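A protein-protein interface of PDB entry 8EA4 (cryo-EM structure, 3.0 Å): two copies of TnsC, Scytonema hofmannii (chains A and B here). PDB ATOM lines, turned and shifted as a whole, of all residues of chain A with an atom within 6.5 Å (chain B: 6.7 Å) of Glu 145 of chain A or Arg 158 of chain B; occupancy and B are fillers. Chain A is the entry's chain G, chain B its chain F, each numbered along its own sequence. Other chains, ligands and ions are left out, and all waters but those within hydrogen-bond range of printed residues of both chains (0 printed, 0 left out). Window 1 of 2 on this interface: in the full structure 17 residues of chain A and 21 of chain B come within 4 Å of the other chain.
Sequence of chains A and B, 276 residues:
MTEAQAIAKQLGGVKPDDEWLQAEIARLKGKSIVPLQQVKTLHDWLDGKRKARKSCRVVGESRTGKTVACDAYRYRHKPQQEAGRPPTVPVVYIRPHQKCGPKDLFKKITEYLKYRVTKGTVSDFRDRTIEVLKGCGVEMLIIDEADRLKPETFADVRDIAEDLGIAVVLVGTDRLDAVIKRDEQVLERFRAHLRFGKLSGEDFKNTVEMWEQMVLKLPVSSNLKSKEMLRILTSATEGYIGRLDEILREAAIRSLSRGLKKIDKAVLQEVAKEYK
The backbone carbonyl oxygen (O) of Ala 155 of chain B sits at hydrogen-bond distance from the guanidinium group (NH2) of Arg 148 of chain A (3.3 Å). OE1 of Glu 145 of chain A lies within salt-bridge range of NH2 of Arg 158 of chain B, at 3.6 Å. The guanidinium group (NH2) of Arg 95 of chain A lies within salt-bridge range of the side-chain carboxylate (OD1) of Asp 159 of chain B (2.8 Å). The guanidinium group (NH1) of Arg 175 of chain A lies within salt-bridge range of the side-chain carboxylate (OD1) of Asp 183 of chain B (3.3 Å). The side-chain amide nitrogen of Gln 185 of chain B sits close to the guanidinium group of Arg 175 of chain A, at 3.2 Å.
The side-chain carboxylate (OD1) of Asp 183 of chain B sits close to the backbone NH (N) of Gln 185 of chain B (3.4 Å). NH1 of Arg 189 of chain B lies within hydrogen-bond range of O of Gln 185 of chain B, at 3.0 Å. The backbone carbonyl oxygen of Pro 96 of chain A sits at hydrogen-bond distance from the guanidinium group of Arg 148 of chain A (2.9 Å). OE1 of Glu 145 of chain A is in salt-bridge range of NE of Arg 148 of chain A, 2.7 Å away. N of Glu 145 of chain A is in hydrogen-bond range of O of Val 171 of chain A, 3.3 Å away. The side-chain carboxylate (OD2) of Asp 147 of chain A lies within salt-bridge range of the guanidinium group (NH2) of Arg 175 of chain A.
Ala 155 of chain B touches Gln 98 of chain A. NE2 of Gln 185 of chain B touches OD2 of Asp 147 of chain A (3.96 Å). NH2 of Arg 158 of chain B touches NH2 of Arg 148 of chain A, at 3.8 Å.
Of the printed residues of chain B, Glu 145 of chain A touches Arg 158. Arg 158 of chain B touches just these residues of chain A: Glu 145 (3.6 Å) and Arg 148 (3.8 Å). Of the printed residues of chain A, Asp 183 of chain B touches Arg 175. Of the printed residues of chain B, Arg 95 of chain A touches Asp 159. Of the printed residues of chain B, Arg 175 of chain A touches Asp 183 and Gln 185. Printed residues of chain B within 4 Å of Asp 147 of chain A: Gln 185 (3.96 Å). Leu 187 of chain B touches none of the printed residues of chain A. The nearest printed residue of chain B that does not touch Glu 145 of chain A is Glu 162 of chain B (5.3 Å). The nearest residue of chain A that does not touch Arg 158 of chain B is Arg 175 of chain A (5.2 Å).
Of the 18 printed residues of chain B, 5 touch a printed residue of chain A. Printed residues of chain B that touch a printed residue of chain A: Ala 155, Arg 158, Asp 159, Asp 183 and Gln 185. Among the printed residues, 8 pairs touch across the chains. Among the printed residues, Asp or Glu carboxylates within 4 Å of a Lys or Arg side-chain nitrogen of the other chain: Arg 95 of chain A with Asp 159 of chain B, Glu 145 of chain A with Arg 158 of chain B and Arg 175 of chain A with Asp 183 of chain B.
No position is printed for both chains. Of the 8 pairs that touch across the chains among the printed residues, none has its exchanged pair printed and touching as well.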
ATOM      1  N   TYR A  93     -17.556   4.775  -2.364  1.00  0.00           N
ATOM      2  CA  TYR A  93     -18.279   3.715  -3.097  1.00  0.00           C
ATOM      3  C   TYR A  93     -19.784   3.915  -2.963  1.00  0.00           C
ATOM      4  O   TYR A  93     -20.307   3.929  -1.854  1.00  0.00           O
ATOM      5  CB  TYR A  93     -17.841   2.336  -2.594  1.00  0.00           C
ATOM      6  CG  TYR A  93     -18.694   1.160  -3.034  1.00  0.00           C
ATOM      7  CD1 TYR A  93     -19.805   0.793  -2.274  1.00  0.00           C
ATOM      8  CD2 TYR A  93     -18.387   0.419  -4.172  1.00  0.00           C
ATOM      9  CE1 TYR A  93     -20.636  -0.257  -2.681  1.00  0.00           C
ATOM     10  CE2 TYR A  93     -19.214  -0.639  -4.589  1.00  0.00           C
ATOM     11  CZ  TYR A  93     -20.356  -0.966  -3.847  1.00  0.00           C
ATOM     12  OH  TYR A  93     -21.207  -1.953  -4.224  1.00  0.00           O
ATOM     13  N   ILE A  94     -20.495   4.041  -4.077  1.00  0.00           N
ATOM     14  CA  ILE A  94     -21.947   4.230  -4.089  1.00  0.00           C
ATOM     15  C   ILE A  94     -22.675   3.212  -4.954  1.00  0.00           C
ATOM     16  O   ILE A  94     -22.071   2.630  -5.816  1.00  0.00           O
ATOM     17  CB  ILE A  94     -22.298   5.646  -4.583  1.00  0.00           C
ATOM     18  CG1 ILE A  94     -21.819   5.846  -6.022  1.00  0.00           C
ATOM     19  CG2 ILE A  94     -21.693   6.695  -3.664  1.00  0.00           C
ATOM     20  CD1 ILE A  94     -22.275   7.146  -6.643  1.00  0.00           C
ATOM     21  N   ARG A  95     -23.962   2.983  -4.729  1.00  0.00           N
ATOM     22  CA  ARG A  95     -24.720   2.136  -5.639  1.00  0.00           C
ATOM     23  C   ARG A  95     -26.014   2.862  -5.949  1.00  0.00           C
ATOM     24  O   ARG A  95     -26.815   3.101  -5.056  1.00  0.00           O
ATOM     25  CB  ARG A  95     -25.011   0.772  -5.029  1.00  0.00           C
ATOM     26  CG  ARG A  95     -25.777  -0.181  -5.931  1.00  0.00           C
ATOM     27  CD  ARG A  95     -25.944  -1.519  -5.306  1.00  0.00           C
ATOM     28  NE  ARG A  95     -26.756  -1.449  -4.100  1.00  0.00           N
ATOM     29  CZ  ARG A  95     -26.736  -2.368  -3.114  1.00  0.00           C
ATOM     30  NH1 ARG A  95     -25.946  -3.414  -3.203  1.00  0.00           N
ATOM     31  NH2 ARG A  95     -27.518  -2.218  -2.056  1.00  0.00           N
ATOM     32  N   PRO A  96     -26.256   3.185  -7.225  1.00  0.00           N
ATOM     33  CA  PRO A  96     -27.439   3.937  -7.635  1.00  0.00           C
ATOM     34  C   PRO A  96     -28.720   3.123  -7.608  1.00  0.00           C
ATOM     35  O   PRO A  96     -28.656   1.920  -7.748  1.00  0.00           O
ATOM     36  CB  PRO A  96     -27.088   4.354  -9.068  1.00  0.00           C
ATOM     37  CG  PRO A  96     -26.143   3.298  -9.534  1.00  0.00           C
ATOM     38  CD  PRO A  96     -25.314   2.972  -8.319  1.00  0.00           C
ATOM     39  N   GLN A  98     -32.460   2.313  -9.579  1.00  0.00           N
ATOM     40  CA  GLN A  98     -32.824   2.246 -10.993  1.00  0.00           C
ATOM     41  C   GLN A  98     -33.409   3.583 -11.522  1.00  0.00           C
ATOM     42  O   GLN A  98     -34.063   4.307 -10.778  1.00  0.00           O
ATOM     43  CB  GLN A  98     -33.732   1.027 -11.140  1.00  0.00           C
ATOM     44  CG  GLN A  98     -34.104   0.605 -12.554  1.00  0.00           C
ATOM     45  CD  GLN A  98     -32.931   0.419 -13.500  1.00  0.00           C
ATOM     46  OE1 GLN A  98     -32.301   1.369 -13.920  1.00  0.00           O
ATOM     47  NE2 GLN A  98     -32.608  -0.795 -13.875  1.00  0.00           N
ATOM     48  N   ILE A 143     -18.560   3.330  -8.910  1.00  0.00           N
ATOM     49  CA  ILE A 143     -19.993   3.250  -9.127  1.00  0.00           C
ATOM     50  C   ILE A 143     -20.381   1.838  -9.473  1.00  0.00           C
ATOM     51  O   ILE A 143     -20.075   1.373 -10.541  1.00  0.00           O
ATOM     52  CB  ILE A 143     -20.445   4.202 -10.250  1.00  0.00           C
ATOM     53  CG1 ILE A 143     -20.102   5.651  -9.896  1.00  0.00           C
ATOM     54  CG2 ILE A 143     -21.939   4.049 -10.505  1.00  0.00           C
ATOM     55  CD1 ILE A 143     -20.410   6.641 -10.998  1.00  0.00           C
ATOM     56  N   ASP A 144     -21.119   1.178  -8.601  1.00  0.00           N
ATOM     57  CA  ASP A 144     -21.577  -0.176  -8.842  1.00  0.00           C
ATOM     58  C   ASP A 144     -22.797  -0.155  -9.701  1.00  0.00           C
ATOM     59  O   ASP A 144     -23.456   0.864  -9.761  1.00  0.00           O
ATOM     60  CB  ASP A 144     -21.883  -0.901  -7.528  1.00  0.00           C
ATOM     61  CG  ASP A 144     -21.868  -2.417  -7.673  1.00  0.00           C
ATOM     62  OD1 ASP A 144     -21.814  -2.889  -8.782  1.00  0.00           O
ATOM     63  OD2 ASP A 144     -21.906  -3.090  -6.668  1.00  0.00           O
ATOM     64  N   GLU A 145     -23.106  -1.276 -10.349  1.00  0.00           N
ATOM     65  CA  GLU A 145     -24.235  -1.371 -11.269  1.00  0.00           C
ATOM     66  C   GLU A 145     -24.356  -0.120 -12.102  1.00  0.00           C
ATOM     67  O   GLU A 145     -25.377   0.516 -12.096  1.00  0.00           O
ATOM     68  CB  GLU A 145     -25.537  -1.606 -10.502  1.00  0.00           C
ATOM     69  CG  GLU A 145     -25.572  -2.899  -9.698  1.00  0.00           C
ATOM     70  CD  GLU A 145     -26.946  -3.240  -9.196  1.00  0.00           C
ATOM     71  OE1 GLU A 145     -27.856  -3.274  -9.991  1.00  0.00           O
ATOM     72  OE2 GLU A 145     -27.086  -3.466  -8.020  1.00  0.00           O
ATOM     73  N   ALA A 146     -23.300   0.268 -12.803  1.00  0.00           N
ATOM     74  CA  ALA A 146     -23.289   1.573 -13.453  1.00  0.00           C
ATOM     75  C   ALA A 146     -24.420   1.777 -14.419  1.00  0.00           C
ATOM     76  O   ALA A 146     -24.848   2.894 -14.624  1.00  0.00           O
ATOM     77  CB  ALA A 146     -21.974   1.807 -14.160  1.00  0.00           C
ATOM     78  N   ASP A 147     -24.896   0.712 -15.037  1.00  0.00           N
ATOM     79  CA  ASP A 147     -26.001   0.824 -15.973  1.00  0.00           C
ATOM     80  C   ASP A 147     -27.384   1.173 -15.394  1.00  0.00           C
ATOM     81  O   ASP A 147     -28.350   1.161 -16.131  1.00  0.00           O
ATOM     82  CB  ASP A 147     -26.117  -0.486 -16.749  1.00  0.00           C
ATOM     83  CG  ASP A 147     -26.427  -1.679 -15.855  1.00  0.00           C
ATOM     84  OD1 ASP A 147     -26.355  -1.534 -14.655  1.00  0.00           O
ATOM     85  OD2 ASP A 147     -26.736  -2.725 -16.374  1.00  0.00           O
ATOM     86  N   ARG A 148     -27.506   1.462 -14.100  1.00  0.00           N
ATOM     87  CA  ARG A 148     -28.704   2.057 -13.664  1.00  0.00           C
ATOM     88  C   ARG A 148     -28.771   3.539 -13.938  1.00  0.00           C
ATOM     89  O   ARG A 148     -29.782   4.129 -13.729  1.00  0.00           O
ATOM     90  CB  ARG A 148     -28.871   1.813 -12.171  1.00  0.00           C
ATOM     91  CG  ARG A 148     -29.112   0.362 -11.785  1.00  0.00           C
ATOM     92  CD  ARG A 148     -29.244   0.199 -10.314  1.00  0.00           C
ATOM     93  NE  ARG A 148     -29.543  -1.173  -9.945  1.00  0.00           N
ATOM     94  CZ  ARG A 148     -29.861  -1.580  -8.699  1.00  0.00           C
ATOM     95  NH1 ARG A 148     -29.918  -0.706  -7.719  1.00  0.00           N
ATOM     96  NH2 ARG A 148     -30.118  -2.853  -8.465  1.00  0.00           N
ATOM     97  N   LEU A 149     -27.663   4.126 -14.350  1.00  0.00           N
ATOM     98  CA  LEU A 149     -27.598   5.562 -14.627  1.00  0.00           C
ATOM     99  C   LEU A 149     -28.412   5.862 -15.867  1.00  0.00           C
ATOM    100  O   LEU A 149     -28.392   5.121 -16.822  1.00  0.00           O
ATOM    101  CB  LEU A 149     -26.148   6.023 -14.823  1.00  0.00           C
ATOM    102  CG  LEU A 149     -25.259   5.974 -13.576  1.00  0.00           C
ATOM    103  CD1 LEU A 149     -23.819   6.279 -13.965  1.00  0.00           C
ATOM    104  CD2 LEU A 149     -25.772   6.972 -12.548  1.00  0.00           C
ATOM    105  N   VAL A 171     -18.360  -0.204 -12.490  1.00  0.00           N
ATOM    106  CA  VAL A 171     -18.394  -1.663 -12.310  1.00  0.00           C
ATOM    107  C   VAL A 171     -19.670  -2.226 -12.918  1.00  0.00           C
ATOM    108  O   VAL A 171     -20.755  -1.728 -12.630  1.00  0.00           O
ATOM    109  CB  VAL A 171     -18.275  -2.056 -10.831  1.00  0.00           C
ATOM    110  CG1 VAL A 171     -18.228  -3.565 -10.642  1.00  0.00           C
ATOM    111  CG2 VAL A 171     -17.039  -1.456 -10.183  1.00  0.00           C
ATOM    112  N   GLY A 172     -19.594  -3.270 -13.743  1.00  0.00           N
ATOM    113  CA  GLY A 172     -20.826  -3.898 -14.233  1.00  0.00           C
ATOM    114  C   GLY A 172     -20.739  -5.143 -15.122  1.00  0.00           C
ATOM    115  O   GLY A 172     -19.651  -5.613 -15.403  1.00  0.00           O
ATOM    116  N   ARG A 175     -23.886  -6.052 -20.221  1.00  0.00           N
ATOM    117  CA  ARG A 175     -24.840  -5.113 -20.647  1.00  0.00           C
ATOM    118  C   ARG A 175     -24.329  -3.727 -20.501  1.00  0.00           C
ATOM    119  O   ARG A 175     -24.800  -2.858 -21.159  1.00  0.00           O
ATOM    120  CB  ARG A 175     -26.129  -5.268 -19.852  1.00  0.00           C
ATOM    121  CG  ARG A 175     -27.276  -4.382 -20.314  1.00  0.00           C
ATOM    122  CD  ARG A 175     -28.530  -4.680 -19.576  1.00  0.00           C
ATOM    123  NE  ARG A 175     -28.422  -4.343 -18.165  1.00  0.00           N
ATOM    124  CZ  ARG A 175     -29.271  -4.771 -17.210  1.00  0.00           C
ATOM    125  NH1 ARG A 175     -30.281  -5.547 -17.531  1.00  0.00           N
ATOM    126  NH2 ARG A 175     -29.088  -4.411 -15.953  1.00  0.00           N
ATOM    127  N   LEU A 176     -23.435  -3.464 -19.561  1.00  0.00           N
ATOM    128  CA  LEU A 176     -22.961  -2.092 -19.359  1.00  0.00           C
ATOM    129  C   LEU A 176     -22.330  -1.653 -20.618  1.00  0.00           C
ATOM    130  O   LEU A 176     -22.581  -0.588 -21.059  1.00  0.00           O
ATOM    131  CB  LEU A 176     -21.952  -1.999 -18.208  1.00  0.00           C
ATOM    132  CG  LEU A 176     -21.312  -0.622 -17.995  1.00  0.00           C
ATOM    133  CD1 LEU A 176     -22.397   0.404 -17.705  1.00  0.00           C
ATOM    134  CD2 LEU A 176     -20.309  -0.697 -16.851  1.00  0.00           C
ATOM    135  N   THR B 153     -38.136  -3.344 -12.206  1.00  0.00           N
ATOM    136  CA  THR B 153     -38.406  -3.466 -10.777  1.00  0.00           C
ATOM    137  C   THR B 153     -37.589  -4.518 -10.173  1.00  0.00           C
ATOM    138  O   THR B 153     -37.652  -4.684  -8.992  1.00  0.00           O
ATOM    139  CB  THR B 153     -39.888  -3.768 -10.490  1.00  0.00           C
ATOM    140  OG1 THR B 153     -40.258  -5.002 -11.121  1.00  0.00           O
ATOM    141  CG2 THR B 153     -40.770  -2.648 -11.017  1.00  0.00           C
ATOM    142  N   PHE B 154     -37.030  -5.363 -11.016  1.00  0.00           N
ATOM    143  CA  PHE B 154     -36.228  -6.445 -10.525  1.00  0.00           C
ATOM    144  C   PHE B 154     -34.988  -5.897  -9.856  1.00  0.00           C
ATOM    145  O   PHE B 154     -34.378  -6.561  -9.047  1.00  0.00           O
ATOM    146  CB  PHE B 154     -35.915  -7.401 -11.647  1.00  0.00           C
ATOM    147  CG  PHE B 154     -37.054  -8.315 -11.975  1.00  0.00           C
ATOM    148  CD1 PHE B 154     -37.229  -9.483 -11.273  1.00  0.00           C
ATOM    149  CD2 PHE B 154     -37.934  -8.006 -12.984  1.00  0.00           C
ATOM    150  CE1 PHE B 154     -38.265 -10.332 -11.575  1.00  0.00           C
ATOM    151  CE2 PHE B 154     -38.978  -8.857 -13.294  1.00  0.00           C
ATOM    152  CZ  PHE B 154     -39.145 -10.025 -12.587  1.00  0.00           C
ATOM    153  N   ALA B 155     -34.608  -4.678 -10.196  1.00  0.00           N
ATOM    154  CA  ALA B 155     -33.481  -4.066  -9.536  1.00  0.00           C
ATOM    155  C   ALA B 155     -33.784  -3.906  -8.065  1.00  0.00           C
ATOM    156  O   ALA B 155     -32.908  -4.030  -7.229  1.00  0.00           O
ATOM    157  CB  ALA B 155     -33.166  -2.727 -10.161  1.00  0.00           C
ATOM    158  N   ASP B 156     -35.021  -3.567  -7.744  1.00  0.00           N
ATOM    159  CA  ASP B 156     -35.411  -3.351  -6.353  1.00  0.00           C
ATOM    160  C   ASP B 156     -35.638  -4.657  -5.604  1.00  0.00           C
ATOM    161  O   ASP B 156     -35.443  -4.730  -4.403  1.00  0.00           O
ATOM    162  CB  ASP B 156     -36.679  -2.498  -6.288  1.00  0.00           C
ATOM    163  CG  ASP B 156     -36.438  -1.050  -6.703  1.00  0.00           C
ATOM    164  OD1 ASP B 156     -35.788  -0.344  -5.971  1.00  0.00           O
ATOM    165  OD2 ASP B 156     -36.910  -0.665  -7.745  1.00  0.00           O
ATOM    166  N   VAL B 157     -36.126  -5.669  -6.311  1.00  0.00           N
ATOM    167  CA  VAL B 157     -36.220  -7.013  -5.753  1.00  0.00           C
ATOM    168  C   VAL B 157     -34.863  -7.622  -5.415  1.00  0.00           C
ATOM    169  O   VAL B 157     -34.719  -8.204  -4.373  1.00  0.00           O
ATOM    170  CB  VAL B 157     -36.945  -7.937  -6.750  1.00  0.00           C
ATOM    171  CG1 VAL B 157     -36.883  -9.381  -6.276  1.00  0.00           C
ATOM    172  CG2 VAL B 157     -38.386  -7.486  -6.921  1.00  0.00           C
ATOM    173  N   ARG B 158     -33.874  -7.503  -6.296  1.00  0.00           N
ATOM    174  CA  ARG B 158     -32.532  -7.984  -5.990  1.00  0.00           C
ATOM    175  C   ARG B 158     -31.922  -7.212  -4.847  1.00  0.00           C
ATOM    176  O   ARG B 158     -31.317  -7.782  -3.961  1.00  0.00           O
ATOM    177  CB  ARG B 158     -31.625  -7.868  -7.209  1.00  0.00           C
ATOM    178  CG  ARG B 158     -31.907  -8.878  -8.312  1.00  0.00           C
ATOM    179  CD  ARG B 158     -30.850  -8.858  -9.355  1.00  0.00           C
ATOM    180  NE  ARG B 158     -30.967  -7.692 -10.223  1.00  0.00           N
ATOM    181  CZ  ARG B 158     -30.116  -6.650 -10.220  1.00  0.00           C
ATOM    182  NH1 ARG B 158     -29.093  -6.636  -9.396  1.00  0.00           N
ATOM    183  NH2 ARG B 158     -30.309  -5.638 -11.050  1.00  0.00           N
ATOM    184  N   ASP B 159     -32.093  -5.899  -4.865  1.00  0.00           N
ATOM    185  CA  ASP B 159     -31.501  -5.015  -3.874  1.00  0.00           C
ATOM    186  C   ASP B 159     -31.880  -5.417  -2.471  1.00  0.00           C
ATOM    187  O   ASP B 159     -31.029  -5.486  -1.594  1.00  0.00           O
ATOM    188  CB  ASP B 159     -31.933  -3.568  -4.125  1.00  0.00           C
ATOM    189  CG  ASP B 159     -31.245  -2.577  -3.197  1.00  0.00           C
ATOM    190  OD1 ASP B 159     -30.038  -2.516  -3.214  1.00  0.00           O
ATOM    191  OD2 ASP B 159     -31.933  -1.889  -2.482  1.00  0.00           O
ATOM    192  N   ILE B 160     -33.166  -5.644  -2.246  1.00  0.00           N
ATOM    193  CA  ILE B 160     -33.676  -6.086  -0.959  1.00  0.00           C
ATOM    194  C   ILE B 160     -33.095  -7.435  -0.582  1.00  0.00           C
ATOM    195  O   ILE B 160     -32.645  -7.609   0.524  1.00  0.00           O
ATOM    196  CB  ILE B 160     -35.215  -6.175  -0.974  1.00  0.00           C
ATOM    197  CG1 ILE B 160     -35.831  -4.777  -1.066  1.00  0.00           C
ATOM    198  CG2 ILE B 160     -35.718  -6.901   0.266  1.00  0.00           C
ATOM    199  CD1 ILE B 160     -37.311  -4.779  -1.363  1.00  0.00           C
ATOM    200  N   ALA B 161     -33.182  -8.376  -1.521  1.00  0.00           N
ATOM    201  CA  ALA B 161     -32.709  -9.727  -1.341  1.00  0.00           C
ATOM    202  C   ALA B 161     -31.218  -9.754  -1.007  1.00  0.00           C
ATOM    203  O   ALA B 161     -30.780 -10.684  -0.343  1.00  0.00           O
ATOM    204  CB  ALA B 161     -32.994 -10.526  -2.615  1.00  0.00           C
ATOM    205  N   GLU B 162     -30.428  -8.767  -1.439  1.00  0.00           N
ATOM    206  CA  GLU B 162     -28.983  -8.802  -1.106  1.00  0.00           C
ATOM    207  C   GLU B 162     -28.689  -8.004   0.174  1.00  0.00           C
ATOM    208  O   GLU B 162     -27.819  -8.447   0.950  1.00  0.00           O
ATOM    209  CB  GLU B 162     -28.148  -8.247  -2.261  1.00  0.00           C
ATOM    210  CG  GLU B 162     -28.113  -9.134  -3.497  1.00  0.00           C
ATOM    211  CD  GLU B 162     -27.209  -8.602  -4.572  1.00  0.00           C
ATOM    212  OE1 GLU B 162     -26.834  -7.458  -4.496  1.00  0.00           O
ATOM    213  OE2 GLU B 162     -26.895  -9.342  -5.478  1.00  0.00           O
ATOM    214  N   ASP B 163     -29.390  -6.877   0.362  1.00  0.00           N
ATOM    215  CA  ASP B 163     -29.131  -5.901   1.460  1.00  0.00           C
ATOM    216  C   ASP B 163     -29.650  -6.442   2.800  1.00  0.00           C
ATOM    217  O   ASP B 163     -28.938  -6.292   3.811  1.00  0.00           O
ATOM    218  CB  ASP B 163     -29.793  -4.552   1.164  1.00  0.00           C
ATOM    219  CG  ASP B 163     -29.425  -3.478   2.176  1.00  0.00           C
ATOM    220  OD1 ASP B 163     -28.258  -3.293   2.421  1.00  0.00           O
ATOM    221  OD2 ASP B 163     -30.318  -2.850   2.696  1.00  0.00           O
ATOM    222  N   VAL B 168     -36.317 -14.095  -1.253  1.00  0.00           N
ATOM    223  CA  VAL B 168     -37.402 -13.752  -2.177  1.00  0.00           C
ATOM    224  C   VAL B 168     -37.721 -15.004  -2.955  1.00  0.00           C
ATOM    225  O   VAL B 168     -36.830 -15.622  -3.527  1.00  0.00           O
ATOM    226  CB  VAL B 168     -37.047 -12.596  -3.114  1.00  0.00           C
ATOM    227  CG1 VAL B 168     -38.182 -12.319  -4.100  1.00  0.00           C
ATOM    228  CG2 VAL B 168     -36.788 -11.307  -2.342  1.00  0.00           C
ATOM    229  N   ASP B 183     -32.447 -11.284 -18.610  1.00  0.00           N
ATOM    230  CA  ASP B 183     -31.651 -10.513 -17.661  1.00  0.00           C
ATOM    231  C   ASP B 183     -30.735 -11.408 -16.814  1.00  0.00           C
ATOM    232  O   ASP B 183     -31.140 -11.986 -15.812  1.00  0.00           O
ATOM    233  CB  ASP B 183     -32.603  -9.664 -16.815  1.00  0.00           C
ATOM    234  CG  ASP B 183     -31.893  -8.603 -15.977  1.00  0.00           C
ATOM    235  OD1 ASP B 183     -30.654  -8.498 -16.051  1.00  0.00           O
ATOM    236  OD2 ASP B 183     -32.591  -7.845 -15.282  1.00  0.00           O
ATOM    237  N   GLN B 185     -28.496 -10.755 -14.691  1.00  0.00           N
ATOM    238  CA  GLN B 185     -28.358 -10.380 -13.279  1.00  0.00           C
ATOM    239  C   GLN B 185     -29.401 -11.095 -12.443  1.00  0.00           C
ATOM    240  O   GLN B 185     -29.091 -11.559 -11.350  1.00  0.00           O
ATOM    241  CB  GLN B 185     -28.526  -8.877 -13.016  1.00  0.00           C
ATOM    242  CG  GLN B 185     -27.242  -8.049 -13.000  1.00  0.00           C
ATOM    243  CD  GLN B 185     -26.909  -7.470 -14.353  1.00  0.00           C
ATOM    244  OE1 GLN B 185     -26.653  -8.169 -15.311  1.00  0.00           O
ATOM    245  NE2 GLN B 185     -26.824  -6.200 -14.478  1.00  0.00           N
ATOM    246  N   VAL B 186     -30.629 -11.189 -12.933  1.00  0.00           N
ATOM    247  CA  VAL B 186     -31.701 -11.827 -12.203  1.00  0.00           C
ATOM    248  C   VAL B 186     -31.690 -13.292 -12.281  1.00  0.00           C
ATOM    249  O   VAL B 186     -31.981 -13.920 -11.358  1.00  0.00           O
ATOM    250  CB  VAL B 186     -33.067 -11.336 -12.724  1.00  0.00           C
ATOM    251  CG1 VAL B 186     -34.201 -12.059 -12.015  1.00  0.00           C
ATOM    252  CG2 VAL B 186     -33.184  -9.832 -12.534  1.00  0.00           C
ATOM    253  N   LEU B 187     -31.466 -13.853 -13.426  1.00  0.00           N
ATOM    254  CA  LEU B 187     -31.498 -15.276 -13.544  1.00  0.00           C
ATOM    255  C   LEU B 187     -30.639 -15.916 -12.544  1.00  0.00           C
ATOM    256  O   LEU B 187     -30.990 -16.943 -12.111  1.00  0.00           O
ATOM    257  CB  LEU B 187     -31.050 -15.711 -14.948  1.00  0.00           C
ATOM    258  CG  LEU B 187     -31.132 -17.215 -15.235  1.00  0.00           C
ATOM    259  CD1 LEU B 187     -31.303 -17.435 -16.732  1.00  0.00           C
ATOM    260  CD2 LEU B 187     -29.873 -17.900 -14.722  1.00  0.00           C
ATOM    261  N   ARG B 189     -29.582 -14.807  -9.470  1.00  0.00           N
ATOM    262  CA  ARG B 189     -30.112 -14.813  -8.096  1.00  0.00           C
ATOM    263  C   ARG B 189     -31.165 -15.913  -7.911  1.00  0.00           C
ATOM    264  O   ARG B 189     -31.250 -16.485  -6.833  1.00  0.00           O
ATOM    265  CB  ARG B 189     -30.677 -13.443  -7.684  1.00  0.00           C
ATOM    266  CG  ARG B 189     -29.646 -12.419  -7.169  1.00  0.00           C
ATOM    267  CD  ARG B 189     -28.787 -11.845  -8.300  1.00  0.00           C
ATOM    268  NE  ARG B 189     -27.873 -10.774  -7.855  1.00  0.00           N
ATOM    269  CZ  ARG B 189     -26.995 -10.126  -8.594  1.00  0.00           C
ATOM    270  NH1 ARG B 189     -26.763 -10.376  -9.835  1.00  0.00           N
ATOM    271  NH2 ARG B 189     -26.306  -9.165  -8.103  1.00  0.00           N
ATOM    272  N   PHE B 190     -31.946 -16.234  -8.949  1.00  0.00           N
ATOM    273  CA  PHE B 190     -33.170 -17.047  -8.872  1.00  0.00           C
ATOM    274  C   PHE B 190     -33.097 -18.372  -9.645  1.00  0.00           C
ATOM    275  O   PHE B 190     -34.103 -18.863 -10.152  1.00  0.00           O
ATOM    276  CB  PHE B 190     -34.377 -16.193  -9.289  1.00  0.00           C
ATOM    277  CG  PHE B 190     -34.637 -15.026  -8.370  1.00  0.00           C
ATOM    278  CD1 PHE B 190     -34.039 -13.784  -8.609  1.00  0.00           C
ATOM    279  CD2 PHE B 190     -35.472 -15.176  -7.262  1.00  0.00           C
ATOM    280  CE1 PHE B 190     -34.268 -12.698  -7.759  1.00  0.00           C
ATOM    281  CE2 PHE B 190     -35.699 -14.097  -6.406  1.00  0.00           C
ATOM    282  CZ  PHE B 190     -35.095 -12.856  -6.646  1.00  0.00           C
